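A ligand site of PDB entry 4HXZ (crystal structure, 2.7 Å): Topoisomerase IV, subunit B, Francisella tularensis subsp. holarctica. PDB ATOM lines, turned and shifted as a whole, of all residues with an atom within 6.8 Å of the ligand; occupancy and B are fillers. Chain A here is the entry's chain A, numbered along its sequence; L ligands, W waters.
The side-chain carboxylate of Glu 45 lies within salt-bridge range of the guanidinium group of Arg 71 (2.8 Å).
The side-chain carboxylate (OD1) of Asp 68 lies within hydrogen-bond range of the backbone NH (N) of Gly 70 (2.8 Å).
N of Asp 68 lies within hydrogen-bond range of O of Thr 162 (3.1 Å).
OD2 of Asp 68 lies within hydrogen-bond range of OG of Ser 42 (3.0 Å).
The backbone carbonyl oxygen of Gly 72 sits at hydrogen-bond distance from the guanidinium group of Arg 131, at 2.8 Å.
N of Val 66 lies within hydrogen-bond range of O of Ile 164 (3.0 Å).
N of Met 73 sits at hydrogen-bond distance from OG1 of Thr 162, 2.8 Å away.
The side-chain amide nitrogen (ND2) of Asn 41 sits at hydrogen-bond distance from the backbone carbonyl oxygen (O) of Glu 37 (2.9 Å).
Water W1 lies within hydrogen-bond range of N2 of the ligand, OD1 of Asp 68, OG1 of Thr 162 and N of Gly 72.
Water W2 bridges the backbone carbonyl oxygen of Asn 41 (2.7 Å) and a nitrogen (N1) of the ligand (3.2 Å).
The side-chain carboxylate of Glu 45 lies close to a sulfur (S1) of the ligand (3.4 Å).
Merely in contact with the ligand: Ile 38, Asn 41, Ser 42, Val 66, Met 73, Pro 74, Val 115 and Ile 164.
Hydrophobic or aromatic side chains that line the ligand: Ile 38, Val 66, Met 73, Pro 74, Val 115 and Ile 164.
Of the 26 residues printed, 12 come within 4 Å of the ligand.
A nitrogen (N2) of the ligand lies within hydrogen-bond range of the side-chain hydroxyl (OG1) of Thr 162, 3.4 Å away.
The backbone NH (N) of Gly 72 sits close to a sulfur (S1) of the ligand.
OD2 of Asp 68 sits at hydrogen-bond distance from N3 of the ligand (2.9 Å).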
ATOM      1  N   GLU A  37      -9.875   7.224  13.126  1.00  0.00           N
ATOM      2  CA  GLU A  37      -9.019   6.872  12.014  1.00  0.00           C
ATOM      3  C   GLU A  37      -8.792   8.108  11.168  1.00  0.00           C
ATOM      4  O   GLU A  37      -7.669   8.391  10.755  1.00  0.00           O
ATOM      5  CB  GLU A  37      -9.614   5.728  11.201  1.00  0.00           C
ATOM      6  CG  GLU A  37      -9.016   5.532   9.805  1.00  0.00           C
ATOM      7  CD  GLU A  37      -7.534   5.175   9.795  1.00  0.00           C
ATOM      8  OE1 GLU A  37      -7.089   4.454  10.720  1.00  0.00           O
ATOM      9  OE2 GLU A  37      -6.810   5.607   8.861  1.00  0.00           O
ATOM     10  N   ILE A  38      -9.852   8.879  10.961  1.00  0.00           N
ATOM     11  CA  ILE A  38      -9.759  10.089  10.159  1.00  0.00           C
ATOM     12  C   ILE A  38      -8.986  11.197  10.894  1.00  0.00           C
ATOM     13  O   ILE A  38      -8.193  11.913  10.274  1.00  0.00           O
ATOM     14  CB  ILE A  38     -11.160  10.522   9.660  1.00  0.00           C
ATOM     15  CG1 ILE A  38     -11.600   9.537   8.592  1.00  0.00           C
ATOM     16  CG2 ILE A  38     -11.153  11.918   9.069  1.00  0.00           C
ATOM     17  CD1 ILE A  38     -13.075   9.546   8.364  1.00  0.00           C
ATOM     18  N   ILE A  39      -9.194  11.325  12.204  1.00  0.00           N
ATOM     19  CA  ILE A  39      -8.387  12.235  12.995  1.00  0.00           C
ATOM     20  C   ILE A  39      -6.924  11.828  12.914  1.00  0.00           C
ATOM     21  O   ILE A  39      -6.063  12.688  12.757  1.00  0.00           O
ATOM     22  CB  ILE A  39      -8.851  12.301  14.448  1.00  0.00           C
ATOM     23  CG1 ILE A  39     -10.235  12.933  14.532  1.00  0.00           C
ATOM     24  CG2 ILE A  39      -7.843  13.042  15.317  1.00  0.00           C
ATOM     25  CD1 ILE A  39     -10.960  12.584  15.803  1.00  0.00           C
ATOM     26  N   ASP A  40      -6.634  10.543  12.978  1.00  0.00           N
ATOM     27  CA  ASP A  40      -5.257  10.078  12.859  1.00  0.00           C
ATOM     28  C   ASP A  40      -4.607  10.627  11.572  1.00  0.00           C
ATOM     29  O   ASP A  40      -3.463  11.082  11.590  1.00  0.00           O
ATOM     30  CB  ASP A  40      -5.192   8.543  12.888  1.00  0.00           C
ATOM     31  CG  ASP A  40      -5.454   7.951  14.295  1.00  0.00           C
ATOM     32  OD1 ASP A  40      -5.436   6.686  14.376  1.00  0.00           O
ATOM     33  OD2 ASP A  40      -5.663   8.713  15.307  1.00  0.00           O
ATOM     34  N   ASN A  41      -5.358  10.590  10.472  1.00  0.00           N
ATOM     35  CA  ASN A  41      -4.897  11.157   9.209  1.00  0.00           C
ATOM     36  C   ASN A  41      -4.654  12.655   9.221  1.00  0.00           C
ATOM     37  O   ASN A  41      -3.620  13.124   8.716  1.00  0.00           O
ATOM     38  CB  ASN A  41      -5.844  10.791   8.119  1.00  0.00           C
ATOM     39  CG  ASN A  41      -5.601   9.405   7.617  1.00  0.00           C
ATOM     40  OD1 ASN A  41      -4.966   9.231   6.572  1.00  0.00           O
ATOM     41  ND2 ASN A  41      -6.045   8.385   8.387  1.00  0.00           N
ATOM     42  N   SER A  42      -5.577  13.423   9.797  1.00  0.00           N
ATOM     43  CA  SER A  42      -5.313  14.821   9.993  1.00  0.00           C
ATOM     44  C   SER A  42      -4.076  14.946  10.833  1.00  0.00           C
ATOM     45  O   SER A  42      -3.197  15.763  10.519  1.00  0.00           O
ATOM     46  CB  SER A  42      -6.470  15.496  10.695  1.00  0.00           C
ATOM     47  OG  SER A  42      -7.643  15.458   9.910  1.00  0.00           O
ATOM     48  N   VAL A  43      -3.991  14.119  11.884  1.00  0.00           N
ATOM     49  CA  VAL A  43      -2.885  14.263  12.852  1.00  0.00           C
ATOM     50  C   VAL A  43      -1.512  14.028  12.241  1.00  0.00           C
ATOM     51  O   VAL A  43      -0.557  14.691  12.630  1.00  0.00           O
ATOM     52  CB  VAL A  43      -3.061  13.422  14.122  1.00  0.00           C
ATOM     53  CG1 VAL A  43      -1.713  13.161  14.785  1.00  0.00           C
ATOM     54  CG2 VAL A  43      -4.004  14.122  15.084  1.00  0.00           C
ATOM     55  N   ASP A  44      -1.417  13.095  11.290  1.00  0.00           N
ATOM     56  CA  ASP A  44      -0.226  12.937  10.468  1.00  0.00           C
ATOM     57  C   ASP A  44       0.188  14.281   9.851  1.00  0.00           C
ATOM     58  O   ASP A  44       1.363  14.673   9.946  1.00  0.00           O
ATOM     59  CB  ASP A  44      -0.482  11.925   9.349  1.00  0.00           C
ATOM     60  CG  ASP A  44      -0.399  10.466   9.821  1.00  0.00           C
ATOM     61  OD1 ASP A  44      -0.151  10.196  11.026  1.00  0.00           O
ATOM     62  OD2 ASP A  44      -0.576   9.572   8.950  1.00  0.00           O
ATOM     63  N   GLU A  45      -0.756  15.013   9.260  1.00  0.00           N
ATOM     64  CA  GLU A  45      -0.404  16.304   8.682  1.00  0.00           C
ATOM     65  C   GLU A  45       0.056  17.279   9.741  1.00  0.00           C
ATOM     66  O   GLU A  45       0.961  18.050   9.499  1.00  0.00           O
ATOM     67  CB  GLU A  45      -1.530  16.880   7.840  1.00  0.00           C
ATOM     68  CG  GLU A  45      -1.650  16.227   6.468  1.00  0.00           C
ATOM     69  CD  GLU A  45      -0.460  16.530   5.554  1.00  0.00           C
ATOM     70  OE1 GLU A  45      -0.358  17.645   5.004  1.00  0.00           O
ATOM     71  OE2 GLU A  45       0.394  15.643   5.377  1.00  0.00           O
ATOM     72  N   VAL A  66     -14.876  15.624   9.439  1.00  0.00           N
ATOM     73  CA  VAL A  66     -13.578  15.977   9.981  1.00  0.00           C
ATOM     74  C   VAL A  66     -12.833  16.763   8.911  1.00  0.00           C
ATOM     75  O   VAL A  66     -12.699  16.273   7.796  1.00  0.00           O
ATOM     76  CB  VAL A  66     -12.742  14.716  10.321  1.00  0.00           C
ATOM     77  CG1 VAL A  66     -11.292  15.103  10.567  1.00  0.00           C
ATOM     78  CG2 VAL A  66     -13.314  13.922  11.494  1.00  0.00           C
ATOM     79  N   ALA A  67     -12.364  17.969   9.231  1.00  0.00           N
ATOM     80  CA  ALA A  67     -11.650  18.851   8.280  1.00  0.00           C
ATOM     81  C   ALA A  67     -10.317  19.353   8.854  1.00  0.00           C
ATOM     82  O   ALA A  67     -10.157  19.517  10.091  1.00  0.00           O
ATOM     83  CB  ALA A  67     -12.531  20.017   7.906  1.00  0.00           C
ATOM     84  N   ASP A  68      -9.343  19.612   7.968  1.00  0.00           N
ATOM     85  CA  ASP A  68      -8.033  20.142   8.392  1.00  0.00           C
ATOM     86  C   ASP A  68      -7.465  21.083   7.342  1.00  0.00           C
ATOM     87  O   ASP A  68      -7.866  21.012   6.175  1.00  0.00           O
ATOM     88  CB  ASP A  68      -7.058  19.019   8.709  1.00  0.00           C
ATOM     89  CG  ASP A  68      -6.623  18.244   7.472  1.00  0.00           C
ATOM     90  OD1 ASP A  68      -6.114  18.859   6.519  1.00  0.00           O
ATOM     91  OD2 ASP A  68      -6.744  16.997   7.477  1.00  0.00           O
ATOM     92  N   GLY A  70      -4.368  21.026   6.294  1.00  0.00           N
ATOM     93  CA  GLY A  70      -3.167  20.365   5.807  1.00  0.00           C
ATOM     94  C   GLY A  70      -2.992  20.579   4.322  1.00  0.00           C
ATOM     95  O   GLY A  70      -3.696  21.414   3.716  1.00  0.00           O
ATOM     96  N   ARG A  71      -2.076  19.823   3.729  1.00  0.00           N
ATOM     97  CA  ARG A  71      -1.735  19.942   2.312  1.00  0.00           C
ATOM     98  C   ARG A  71      -2.837  19.552   1.369  1.00  0.00           C
ATOM     99  O   ARG A  71      -2.853  20.022   0.230  1.00  0.00           O
ATOM    100  CB  ARG A  71      -0.501  19.131   1.939  1.00  0.00           C
ATOM    101  CG  ARG A  71       0.805  19.791   2.342  1.00  0.00           C
ATOM    102  CD  ARG A  71       1.948  18.799   2.242  1.00  0.00           C
ATOM    103  NE  ARG A  71       1.822  17.687   3.192  1.00  0.00           N
ATOM    104  CZ  ARG A  71       2.587  16.596   3.167  1.00  0.00           C
ATOM    105  NH1 ARG A  71       3.540  16.440   2.256  1.00  0.00           N
ATOM    106  NH2 ARG A  71       2.395  15.649   4.081  1.00  0.00           N
ATOM    107  N   GLY A  72      -3.737  18.675   1.808  1.00  0.00           N
ATOM    108  CA  GLY A  72      -4.848  18.201   0.942  1.00  0.00           C
ATOM    109  C   GLY A  72      -4.491  16.938   0.182  1.00  0.00           C
ATOM    110  O   GLY A  72      -3.575  16.943  -0.640  1.00  0.00           O
ATOM    111  N   MET A  73      -5.206  15.845   0.476  1.00  0.00           N
ATOM    112  CA  MET A  73      -5.083  14.562  -0.244  1.00  0.00           C
ATOM    113  C   MET A  73      -4.716  14.669  -1.746  1.00  0.00           C
ATOM    114  O   MET A  73      -5.379  15.417  -2.491  1.00  0.00           O
ATOM    115  CB  MET A  73      -6.369  13.757  -0.141  1.00  0.00           C
ATOM    116  CG  MET A  73      -6.683  13.230   1.238  1.00  0.00           C
ATOM    117  SD  MET A  73      -7.959  11.952   1.184  1.00  0.00           S
ATOM    118  CE  MET A  73      -7.089  10.641   0.344  1.00  0.00           C
ATOM    119  N   PRO A  74      -3.713  13.879  -2.192  1.00  0.00           N
ATOM    120  CA  PRO A  74      -3.207  13.913  -3.552  1.00  0.00           C
ATOM    121  C   PRO A  74      -4.292  13.557  -4.541  1.00  0.00           C
ATOM    122  O   PRO A  74      -5.232  12.813  -4.202  1.00  0.00           O
ATOM    123  CB  PRO A  74      -2.133  12.825  -3.566  1.00  0.00           C
ATOM    124  CG  PRO A  74      -1.816  12.564  -2.142  1.00  0.00           C
ATOM    125  CD  PRO A  74      -3.136  12.741  -1.461  1.00  0.00           C
ATOM    126  N   ILE A  89      -6.555   5.574  -2.314  1.00  0.00           N
ATOM    127  CA  ILE A  89      -6.537   5.491  -0.877  1.00  0.00           C
ATOM    128  C   ILE A  89      -7.922   5.146  -0.358  1.00  0.00           C
ATOM    129  O   ILE A  89      -8.056   4.418   0.619  1.00  0.00           O
ATOM    130  CB  ILE A  89      -6.092   6.854  -0.286  1.00  0.00           C
ATOM    131  CG1 ILE A  89      -4.591   7.078  -0.519  1.00  0.00           C
ATOM    132  CG2 ILE A  89      -6.476   6.989   1.187  1.00  0.00           C
ATOM    133  CD1 ILE A  89      -4.230   8.503  -0.864  1.00  0.00           C
ATOM    134  N   MET A  90      -8.946   5.654  -1.036  1.00  0.00           N
ATOM    135  CA  MET A  90     -10.321   5.503  -0.557  1.00  0.00           C
ATOM    136  C   MET A  90     -10.967   4.146  -0.865  1.00  0.00           C
ATOM    137  O   MET A  90     -11.730   3.625  -0.053  1.00  0.00           O
ATOM    138  CB  MET A  90     -11.209   6.622  -1.081  1.00  0.00           C
ATOM    139  CG  MET A  90     -11.010   7.971  -0.382  1.00  0.00           C
ATOM    140  SD  MET A  90     -11.644   8.071   1.323  1.00  0.00           S
ATOM    141  CE  MET A  90     -11.566   9.859   1.542  1.00  0.00           C
ATOM    142  N   GLY A 114      -5.965   2.602   7.660  1.00  0.00           N
ATOM    143  CA  GLY A 114      -6.195   3.411   6.484  1.00  0.00           C
ATOM    144  C   GLY A 114      -7.640   3.865   6.437  1.00  0.00           C
ATOM    145  O   GLY A 114      -8.534   3.181   6.936  1.00  0.00           O
ATOM    146  N   VAL A 115      -7.865   5.025   5.824  1.00  0.00           N
ATOM    147  CA  VAL A 115      -9.182   5.635   5.742  1.00  0.00           C
ATOM    148  C   VAL A 115     -10.186   4.823   4.943  1.00  0.00           C
ATOM    149  O   VAL A 115     -11.377   4.936   5.162  1.00  0.00           O
ATOM    150  CB  VAL A 115      -9.134   7.097   5.235  1.00  0.00           C
ATOM    151  CG1 VAL A 115      -8.984   7.153   3.719  1.00  0.00           C
ATOM    152  CG2 VAL A 115     -10.351   7.878   5.721  1.00  0.00           C
ATOM    153  N   ARG A 131      -6.231  21.924  -3.073  1.00  0.00           N
ATOM    154  CA  ARG A 131      -4.832  21.859  -3.466  1.00  0.00           C
ATOM    155  C   ARG A 131      -4.769  22.692  -4.733  1.00  0.00           C
ATOM    156  O   ARG A 131      -5.736  22.669  -5.535  1.00  0.00           O
ATOM    157  CB  ARG A 131      -4.462  20.485  -3.968  1.00  0.00           C
ATOM    158  CG  ARG A 131      -4.047  19.469  -2.948  1.00  0.00           C
ATOM    159  CD  ARG A 131      -3.661  18.182  -3.645  1.00  0.00           C
ATOM    160  NE  ARG A 131      -2.302  18.260  -4.148  1.00  0.00           N
ATOM    161  CZ  ARG A 131      -1.214  17.962  -3.442  1.00  0.00           C
ATOM    162  NH1 ARG A 131      -1.320  17.574  -2.178  1.00  0.00           N
ATOM    163  NH2 ARG A 131      -0.037  18.054  -3.997  1.00  0.00           N
ATOM    164  N   GLY A 161      -6.262  22.037   2.152  1.00  0.00           N
ATOM    165  CA  GLY A 161      -6.811  21.100   3.158  1.00  0.00           C
ATOM    166  C   GLY A 161      -7.608  19.910   2.640  1.00  0.00           C
ATOM    167  O   GLY A 161      -7.916  19.801   1.459  1.00  0.00           O
ATOM    168  N   THR A 162      -7.959  19.009   3.546  1.00  0.00           N
ATOM    169  CA  THR A 162      -8.800  17.837   3.229  1.00  0.00           C
ATOM    170  C   THR A 162      -9.995  17.895   4.132  1.00  0.00           C
ATOM    171  O   THR A 162      -9.848  18.156   5.331  1.00  0.00           O
ATOM    172  CB  THR A 162      -8.051  16.503   3.498  1.00  0.00           C
ATOM    173  OG1 THR A 162      -6.965  16.375   2.573  1.00  0.00           O
ATOM    174  CG2 THR A 162      -8.983  15.324   3.332  1.00  0.00           C
ATOM    175  N   LYS A 163     -11.173  17.658   3.549  1.00  0.00           N
ATOM    176  CA  LYS A 163     -12.445  17.611   4.291  1.00  0.00           C
ATOM    177  C   LYS A 163     -13.273  16.343   3.928  1.00  0.00           C
ATOM    178  O   LYS A 163     -13.657  16.177   2.783  1.00  0.00           O
ATOM    179  CB  LYS A 163     -13.237  18.904   4.060  1.00  0.00           C
ATOM    180  CG  LYS A 163     -14.714  18.862   4.446  1.00  0.00           C
ATOM    181  CD  LYS A 163     -15.159  20.188   5.056  1.00  0.00           C
ATOM    182  CE  LYS A 163     -15.848  21.128   4.066  1.00  0.00           C
ATOM    183  NZ  LYS A 163     -15.608  22.562   4.421  1.00  0.00           N
ATOM    184  N   ILE A 164     -13.525  15.476   4.910  1.00  0.00           N
ATOM    185  CA  ILE A 164     -14.279  14.224   4.710  1.00  0.00           C
ATOM    186  C   ILE A 164     -15.568  14.181   5.538  1.00  0.00           C
ATOM    187  O   ILE A 164     -15.510  14.338   6.769  1.00  0.00           O
ATOM    188  CB  ILE A 164     -13.429  12.995   5.104  1.00  0.00           C
ATOM    189  CG1 ILE A 164     -12.196  12.851   4.193  1.00  0.00           C
ATOM    190  CG2 ILE A 164     -14.270  11.736   5.092  1.00  0.00           C
ATOM    191  CD1 ILE A 164     -11.004  12.189   4.860  1.00  0.00           C
HETATM  192  O1  LIG L   1      -8.379  10.545   5.740  1.00  0.00           O
HETATM  193  C1  LIG L   1      -7.370  10.966   5.157  1.00  0.00           C
HETATM  194  C2  LIG L   1      -6.888  12.368   5.337  1.00  0.00           C
HETATM  195  C3  LIG L   1      -7.424  13.447   6.183  1.00  0.00           C
HETATM  196  C4  LIG L   1      -8.621  13.387   7.089  1.00  0.00           C
HETATM  197  C5  LIG L   1      -9.290  14.731   7.197  1.00  0.00           C
HETATM  198  C6  LIG L   1      -5.703  12.883   4.639  1.00  0.00           C
HETATM  199  C7  LIG L   1      -4.686  12.410   3.674  1.00  0.00           C
HETATM  200  O2  LIG L   1      -4.689  11.135   3.183  1.00  0.00           O
HETATM  201  C8  LIG L   1      -3.410  10.533   2.911  1.00  0.00           C
HETATM  202  N1  LIG L   1      -3.722  13.293   3.304  1.00  0.00           N
HETATM  203  C9  LIG L   1      -3.642  14.584   3.743  1.00  0.00           C
HETATM  204  N2  LIG L   1      -4.572  15.058   4.645  1.00  0.00           N
HETATM  205  C10 LIG L   1      -5.588  14.278   5.111  1.00  0.00           C
HETATM  206  N3  LIG L   1      -6.604  14.519   5.982  1.00  0.00           N
HETATM  207  S1  LIG L   1      -2.358  15.570   3.172  1.00  0.00           S
HETATM  208  C11 LIG L   1      -1.198  14.564   2.395  1.00  0.00           C
HETATM  209  C12 LIG L   1      -0.885  13.300   2.920  1.00  0.00           C
HETATM  210  C13 LIG L   1       0.052  12.524   2.245  1.00  0.00           C
HETATM  211  C14 LIG L   1       0.656  12.983   1.067  1.00  0.00           C
HETATM  212  N4  LIG L   1       0.344  14.190   0.578  1.00  0.00           N
HETATM  213  C15 LIG L   1      -0.557  14.967   1.207  1.00  0.00           C
HETATM  214  O   HOH W   1      -5.052  17.737   4.184  1.00  0.00           O
HETATM  215  O   HOH W   2      -2.772  12.423   6.247  1.00  0.00           O
